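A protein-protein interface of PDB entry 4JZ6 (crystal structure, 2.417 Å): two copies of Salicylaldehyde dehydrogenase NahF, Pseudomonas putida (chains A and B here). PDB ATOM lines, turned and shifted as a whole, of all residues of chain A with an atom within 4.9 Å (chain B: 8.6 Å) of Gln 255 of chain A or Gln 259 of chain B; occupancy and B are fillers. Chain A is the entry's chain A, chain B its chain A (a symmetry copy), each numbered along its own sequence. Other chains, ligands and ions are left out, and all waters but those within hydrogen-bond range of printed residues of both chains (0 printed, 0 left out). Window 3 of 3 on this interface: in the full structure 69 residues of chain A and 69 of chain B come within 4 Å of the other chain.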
ATOM      1  N   SER A 251      33.186  10.667   4.011  1.00  0.00           N
ATOM      2  CA  SER A 251      32.127   9.966   4.731  1.00  0.00           C
ATOM      3  C   SER A 251      32.287   8.451   4.601  1.00  0.00           C
ATOM      4  O   SER A 251      32.222   7.717   5.589  1.00  0.00           O
ATOM      5  CB  SER A 251      30.750  10.390   4.220  1.00  0.00           C
ATOM      6  OG  SER A 251      29.728   9.624   4.836  1.00  0.00           O
ATOM      7  N   ILE A 252      32.510   7.998   3.373  1.00  0.00           N
ATOM      8  CA  ILE A 252      32.717   6.585   3.097  1.00  0.00           C
ATOM      9  C   ILE A 252      33.908   6.014   3.871  1.00  0.00           C
ATOM     10  O   ILE A 252      33.804   4.935   4.458  1.00  0.00           O
ATOM     11  CB  ILE A 252      32.878   6.348   1.592  1.00  0.00           C
ATOM     12  CG1 ILE A 252      31.629   6.839   0.861  1.00  0.00           C
ATOM     13  CG2 ILE A 252      33.113   4.880   1.301  1.00  0.00           C
ATOM     14  CD1 ILE A 252      31.707   6.687  -0.639  1.00  0.00           C
ATOM     15  N   ILE A 253      35.026   6.740   3.884  1.00  0.00           N
ATOM     16  CA  ILE A 253      36.189   6.346   4.683  1.00  0.00           C
ATOM     17  C   ILE A 253      35.822   6.216   6.163  1.00  0.00           C
ATOM     18  O   ILE A 253      36.152   5.216   6.809  1.00  0.00           O
ATOM     19  CB  ILE A 253      37.391   7.328   4.498  1.00  0.00           C
ATOM     20  CG1 ILE A 253      38.443   6.727   3.565  1.00  0.00           C
ATOM     21  CG2 ILE A 253      38.071   7.630   5.808  1.00  0.00           C
ATOM     22  CD1 ILE A 253      38.073   6.782   2.117  1.00  0.00           C
ATOM     23  N   ALA A 254      35.115   7.214   6.685  1.00  0.00           N
ATOM     24  CA  ALA A 254      34.771   7.242   8.102  1.00  0.00           C
ATOM     25  C   ALA A 254      33.805   6.118   8.446  1.00  0.00           C
ATOM     26  O   ALA A 254      33.904   5.512   9.509  1.00  0.00           O
ATOM     27  CB  ALA A 254      34.185   8.593   8.480  1.00  0.00           C
ATOM     28  N   GLN A 255      32.877   5.841   7.537  1.00  0.00           N
ATOM     29  CA  GLN A 255      31.946   4.731   7.713  1.00  0.00           C
ATOM     30  C   GLN A 255      32.682   3.400   7.840  1.00  0.00           C
ATOM     31  O   GLN A 255      32.291   2.533   8.625  1.00  0.00           O
ATOM     32  CB  GLN A 255      30.938   4.684   6.564  1.00  0.00           C
ATOM     33  CG  GLN A 255      29.964   5.843   6.574  1.00  0.00           C
ATOM     34  CD  GLN A 255      29.006   5.826   5.407  1.00  0.00           C
ATOM     35  OE1 GLN A 255      29.060   6.697   4.534  1.00  0.00           O
ATOM     36  NE2 GLN A 255      28.107   4.841   5.386  1.00  0.00           N
ATOM     37  N   LYS A 256      33.761   3.248   7.079  1.00  0.00           N
ATOM     38  CA  LYS A 256      34.554   2.030   7.139  1.00  0.00           C
ATOM     39  C   LYS A 256      35.305   1.965   8.458  1.00  0.00           C
ATOM     40  O   LYS A 256      35.346   0.919   9.109  1.00  0.00           O
ATOM     41  CB  LYS A 256      35.526   1.957   5.960  1.00  0.00           C
ATOM     42  CG  LYS A 256      34.842   1.861   4.604  1.00  0.00           C
ATOM     43  CD  LYS A 256      34.190   0.498   4.401  1.00  0.00           C
ATOM     44  CE  LYS A 256      33.646   0.353   2.982  1.00  0.00           C
ATOM     45  NZ  LYS A 256      32.994  -0.972   2.759  1.00  0.00           N
ATOM     46  N   ALA A 257      35.889   3.087   8.860  1.00  0.00           N
ATOM     47  CA  ALA A 257      36.644   3.128  10.103  1.00  0.00           C
ATOM     48  C   ALA A 257      35.735   2.918  11.320  1.00  0.00           C
ATOM     49  O   ALA A 257      36.173   2.419  12.365  1.00  0.00           O
ATOM     50  CB  ALA A 257      37.390   4.427  10.217  1.00  0.00           C
ATOM     51  N   ALA A 258      34.468   3.296  11.179  1.00  0.00           N
ATOM     52  CA  ALA A 258      33.503   3.101  12.251  1.00  0.00           C
ATOM     53  C   ALA A 258      33.222   1.618  12.484  1.00  0.00           C
ATOM     54  O   ALA A 258      32.972   1.198  13.615  1.00  0.00           O
ATOM     55  CB  ALA A 258      32.225   3.843  11.951  1.00  0.00           C
ATOM     56  N   GLN A 259      33.274   0.824  11.418  1.00  0.00           N
ATOM     57  CA  GLN A 259      33.054  -0.616  11.533  1.00  0.00           C
ATOM     58  C   GLN A 259      34.155  -1.268  12.367  1.00  0.00           C
ATOM     59  O   GLN A 259      33.964  -2.355  12.925  1.00  0.00           O
ATOM     60  CB  GLN A 259      32.971  -1.271  10.151  1.00  0.00           C
ATOM     61  CG  GLN A 259      31.871  -0.712   9.265  1.00  0.00           C
ATOM     62  CD  GLN A 259      31.874  -1.328   7.880  1.00  0.00           C
ATOM     63  OE1 GLN A 259      32.050  -2.538   7.725  1.00  0.00           O
ATOM     64  NE2 GLN A 259      31.683  -0.495   6.860  1.00  0.00           N
ATOM     65  N   ASP B 230      19.089   7.472  15.718  1.00  0.00           N
ATOM     66  CA  ASP B 230      19.252   7.771  14.294  1.00  0.00           C
ATOM     67  C   ASP B 230      18.700   9.143  13.939  1.00  0.00           C
ATOM     68  O   ASP B 230      19.322   9.891  13.187  1.00  0.00           O
ATOM     69  CB  ASP B 230      18.563   6.718  13.424  1.00  0.00           C
ATOM     70  CG  ASP B 230      19.170   5.336  13.580  1.00  0.00           C
ATOM     71  OD1 ASP B 230      20.340   5.230  14.007  1.00  0.00           O
ATOM     72  OD2 ASP B 230      18.470   4.349  13.266  1.00  0.00           O
ATOM     73  N   ILE B 233      21.040  11.859  15.412  1.00  0.00           N
ATOM     74  CA  ILE B 233      22.309  11.915  14.697  1.00  0.00           C
ATOM     75  C   ILE B 233      22.110  12.543  13.323  1.00  0.00           C
ATOM     76  O   ILE B 233      22.951  13.319  12.861  1.00  0.00           O
ATOM     77  CB  ILE B 233      22.929  10.507  14.550  1.00  0.00           C
ATOM     78  CG1 ILE B 233      23.301   9.947  15.924  1.00  0.00           C
ATOM     79  CG2 ILE B 233      24.160  10.544  13.656  1.00  0.00           C
ATOM     80  CD1 ILE B 233      23.550   8.460  15.910  1.00  0.00           C
ATOM     81  N   SER B 234      20.987  12.220  12.685  1.00  0.00           N
ATOM     82  CA  SER B 234      20.663  12.754  11.363  1.00  0.00           C
ATOM     83  C   SER B 234      20.119  14.172  11.448  1.00  0.00           C
ATOM     84  O   SER B 234      19.907  14.821  10.426  1.00  0.00           O
ATOM     85  CB  SER B 234      19.643  11.861  10.654  1.00  0.00           C
ATOM     86  OG  SER B 234      20.099  10.524  10.566  1.00  0.00           O
ATOM     87  N   SER B 251      29.913   1.090  17.474  1.00  0.00           N
ATOM     88  CA  SER B 251      30.248   1.054  16.054  1.00  0.00           C
ATOM     89  C   SER B 251      29.073   1.535  15.202  1.00  0.00           C
ATOM     90  O   SER B 251      29.235   2.367  14.306  1.00  0.00           O
ATOM     91  CB  SER B 251      30.658  -0.355  15.628  1.00  0.00           C
ATOM     92  OG  SER B 251      30.869  -0.416  14.227  1.00  0.00           O
ATOM     93  N   ILE B 252      27.891   1.010  15.500  1.00  0.00           N
ATOM     94  CA  ILE B 252      26.676   1.396  14.800  1.00  0.00           C
ATOM     95  C   ILE B 252      26.398   2.897  14.910  1.00  0.00           C
ATOM     96  O   ILE B 252      26.075   3.541  13.910  1.00  0.00           O
ATOM     97  CB  ILE B 252      25.482   0.580  15.305  1.00  0.00           C
ATOM     98  CG1 ILE B 252      25.752  -0.909  15.088  1.00  0.00           C
ATOM     99  CG2 ILE B 252      24.209   0.991  14.593  1.00  0.00           C
ATOM    100  CD1 ILE B 252      24.646  -1.805  15.594  1.00  0.00           C
ATOM    101  N   ILE B 253      26.536   3.452  16.114  1.00  0.00           N
ATOM    102  CA  ILE B 253      26.405   4.897  16.314  1.00  0.00           C
ATOM    103  C   ILE B 253      27.399   5.667  15.441  1.00  0.00           C
ATOM    104  O   ILE B 253      27.026   6.623  14.753  1.00  0.00           O
ATOM    105  CB  ILE B 253      26.563   5.301  17.815  1.00  0.00           C
ATOM    106  CG1 ILE B 253      25.199   5.585  18.447  1.00  0.00           C
ATOM    107  CG2 ILE B 253      27.399   6.545  17.973  1.00  0.00           C
ATOM    108  CD1 ILE B 253      24.417   4.355  18.779  1.00  0.00           C
ATOM    109  N   ALA B 254      28.655   5.227  15.450  1.00  0.00           N
ATOM    110  CA  ALA B 254      29.708   5.923  14.720  1.00  0.00           C
ATOM    111  C   ALA B 254      29.479   5.828  13.219  1.00  0.00           C
ATOM    112  O   ALA B 254      29.723   6.784  12.488  1.00  0.00           O
ATOM    113  CB  ALA B 254      31.072   5.364  15.095  1.00  0.00           C
ATOM    114  N   GLN B 255      29.002   4.674  12.767  1.00  0.00           N
ATOM    115  CA  GLN B 255      28.662   4.488  11.361  1.00  0.00           C
ATOM    116  C   GLN B 255      27.591   5.478  10.910  1.00  0.00           C
ATOM    117  O   GLN B 255      27.636   5.993   9.790  1.00  0.00           O
ATOM    118  CB  GLN B 255      28.213   3.050  11.100  1.00  0.00           C
ATOM    119  CG  GLN B 255      29.333   2.039  11.230  1.00  0.00           C
ATOM    120  CD  GLN B 255      28.876   0.614  11.028  1.00  0.00           C
ATOM    121  OE1 GLN B 255      28.887  -0.190  11.964  1.00  0.00           O
ATOM    122  NE2 GLN B 255      28.483   0.283   9.797  1.00  0.00           N
ATOM    123  N   LYS B 256      26.639   5.759  11.793  1.00  0.00           N
ATOM    124  CA  LYS B 256      25.583   6.709  11.479  1.00  0.00           C
ATOM    125  C   LYS B 256      26.150   8.118  11.436  1.00  0.00           C
ATOM    126  O   LYS B 256      25.844   8.893  10.529  1.00  0.00           O
ATOM    127  CB  LYS B 256      24.447   6.615  12.499  1.00  0.00           C
ATOM    128  CG  LYS B 256      23.724   5.276  12.492  1.00  0.00           C
ATOM    129  CD  LYS B 256      22.872   5.107  11.240  1.00  0.00           C
ATOM    130  CE  LYS B 256      22.028   3.837  11.315  1.00  0.00           C
ATOM    131  NZ  LYS B 256      21.189   3.643  10.095  1.00  0.00           N
ATOM    132  N   ALA B 257      26.989   8.446  12.411  1.00  0.00           N
ATOM    133  CA  ALA B 257      27.578   9.775  12.470  1.00  0.00           C
ATOM    134  C   ALA B 257      28.524  10.022  11.288  1.00  0.00           C
ATOM    135  O   ALA B 257      28.719  11.166  10.856  1.00  0.00           O
ATOM    136  CB  ALA B 257      28.297   9.969  13.774  1.00  0.00           C
ATOM    137  N   ALA B 258      29.107   8.947  10.767  1.00  0.00           N
ATOM    138  CA  ALA B 258      29.988   9.056   9.613  1.00  0.00           C
ATOM    139  C   ALA B 258      29.216   9.466   8.361  1.00  0.00           C
ATOM    140  O   ALA B 258      29.745  10.171   7.501  1.00  0.00           O
ATOM    141  CB  ALA B 258      30.719   7.757   9.385  1.00  0.00           C
ATOM    142  N   GLN B 259      27.961   9.034   8.263  1.00  0.00           N
ATOM    143  CA  GLN B 259      27.122   9.394   7.122  1.00  0.00           C
ATOM    144  C   GLN B 259      26.857  10.898   7.098  1.00  0.00           C
ATOM    145  O   GLN B 259      26.537  11.466   6.046  1.00  0.00           O
ATOM    146  CB  GLN B 259      25.801   8.619   7.145  1.00  0.00           C
ATOM    147  CG  GLN B 259      25.968   7.109   7.129  1.00  0.00           C
ATOM    148  CD  GLN B 259      24.644   6.379   7.234  1.00  0.00           C
ATOM    149  OE1 GLN B 259      23.657   6.762   6.604  1.00  0.00           O
ATOM    150  NE2 GLN B 259      24.614   5.320   8.040  1.00  0.00           N
ATOM    151  N   HIS B 260      27.002  11.539   8.258  1.00  0.00           N
ATOM    152  CA  HIS B 260      26.822  12.986   8.369  1.00  0.00           C
ATOM    153  C   HIS B 260      28.088  13.698   8.849  1.00  0.00           C
ATOM    154  O   HIS B 260      28.028  14.855   9.277  1.00  0.00           O
ATOM    155  CB  HIS B 260      25.646  13.311   9.289  1.00  0.00           C
ATOM    156  CG  HIS B 260      24.380  12.615   8.905  1.00  0.00           C
ATOM    157  ND1 HIS B 260      23.636  12.974   7.804  1.00  0.00           N
ATOM    158  CD2 HIS B 260      23.736  11.562   9.466  1.00  0.00           C
ATOM    159  CE1 HIS B 260      22.585  12.183   7.706  1.00  0.00           C
ATOM    160  NE2 HIS B 260      22.619  11.318   8.702  1.00  0.00           N
ATOM    161  N   LEU B 261      29.222  12.998   8.773  1.00  0.00           N
ATOM    162  CA  LEU B 261      30.534  13.556   9.120  1.00  0.00           C
ATOM    163  C   LEU B 261      30.583  14.183  10.516  1.00  0.00           C
ATOM    164  O   LEU B 261      31.237  15.209  10.713  1.00  0.00           O
ATOM    165  CB  LEU B 261      30.997  14.596   8.078  1.00  0.00           C
ATOM    166  CG  LEU B 261      31.439  14.216   6.655  1.00  0.00           C
ATOM    167  CD1 LEU B 261      32.459  13.088   6.668  1.00  0.00           C
ATOM    168  CD2 LEU B 261      30.253  13.846   5.773  1.00  0.00           C
ATOM    169  N   LYS B 262      29.900  13.578  11.482  1.00  0.00           N
ATOM    170  CA  LYS B 262      29.869  14.149  12.824  1.00  0.00           C
ATOM    171  C   LYS B 262      30.869  13.472  13.744  1.00  0.00           C
ATOM    172  O   LYS B 262      31.017  12.255  13.731  1.00  0.00           O
ATOM    173  CB  LYS B 262      28.456  14.100  13.411  1.00  0.00           C
ATOM    174  CG  LYS B 262      27.409  14.661  12.466  1.00  0.00           C
ATOM    175  CD  LYS B 262      26.297  15.357  13.202  1.00  0.00           C
ATOM    176  CE  LYS B 262      25.230  15.847  12.237  1.00  0.00           C
ATOM    177  NZ  LYS B 262      24.091  16.484  12.959  1.00  0.00           N
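Hydrophobic or aromatic side chains of chain A that line the printed part of chain B: Ala 254 and Ala 258.
Hydrophobic or aromatic side chains of chain B that line the printed part of chain A: Ala 254, Ala 258 and Leu 261.
Among the printed residues, 12 pairs touch across the chains.
Ala 254 of chain A touches just one residue of chain B: Ala 258.
Gln 255 of chain A touches just these residues of chain B: Gln 255 (3.97 Å), Ala 258 (3.4 Å) and Gln 259 (3.6 Å).
Of the printed residues of chain B, Ala 258 of chain A touches Ser 251, Ala 254 and Gln 255.
Printed residues of chain B within 4 Å of Gln 259 of chain A: Ser 251 (3.5 Å) and Gln 255 (3.6 Å).
Of the printed residues of chain A, Ser 251 of chain B touches Ala 258 and Gln 259.
Printed residues of chain A within 4 Å of Gln 255 of chain B: Gln 255 (3.97 Å), Ala 258 (3.4 Å) and Gln 259 (3.6 Å).
Lys 256 of chain B touches none of the printed residues of chain A.
Ala 257 of chain B touches none of the printed residues of chain A.
Of chain A, only Ser 251 and Gln 255 come within 4 Å of Gln 259 of chain B.
The nearest printed residue of chain B that does not touch Gln 259 of chain A is Ala 254 of chain B (6.2 Å).
The side-chain amide oxygen of Gln 255 of chain B lies within hydrogen-bond range of the side-chain hydroxyl of Ser 251 of chain B (3.0 Å).
The side-chain hydroxyl (OG) of Ser 251 of chain A is in hydrogen-bond range of the side-chain amide oxygen (OE1) of Gln 255 of chain A (3.0 Å).
Among the printed residues, pairs that only touch across the chains: Ser 251 of chain A with Gln 259 of chain B (3.5 Å), Ser 251 of chain A with Leu 261 of chain B (3.7 Å), Ala 254 of chain A with Ala 258 of chain B (3.6 Å), Gln 255 of chain A with Gln 255 of chain B (3.97 Å), Gln 255 of chain A with Ala 258 of chain B (3.4 Å), Gln 255 of chain A with Gln 259 of chain B (3.6 Å), Ala 258 of chain A with Ala 254 of chain B (3.6 Å), Ala 258 of chain A with Gln 255 of chain B (3.4 Å), Gln 259 of chain A with Ser 251 of chain B (3.5 Å) and Gln 259 of chain A with Gln 255 of chain B (3.6 Å).
O of Ala 258 of chain A lies within hydrogen-bond range of OG of Ser 251 of chain B, 2.7 Å away.
The backbone carbonyl oxygen (O) of Ala 258 of chain B lies within hydrogen-bond range of the side-chain hydroxyl (OG) of Ser 251 of chain A, 2.7 Å away.
Ser 251 of chain A touches Ala 258 of chain B, and with the chains exchanged Ala 258 of chain A touches Ser 251 of chain B.
Ala 254 of chain A touches Ala 258 of chain B, and with the chains exchanged Ala 258 of chain A touches Ala 254 of chain B.
Gln 255 of chain A touches its own counterpart, Gln 255 of chain B.
Gln 255 of chain A touches Gln 259 of chain B, and with the chains exchanged Gln 259 of chain A touches Gln 255 of chain B.
Of the 12 pairs that touch across the chains among the printed residues, 11 have their exchanged pair printed and touching as well.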
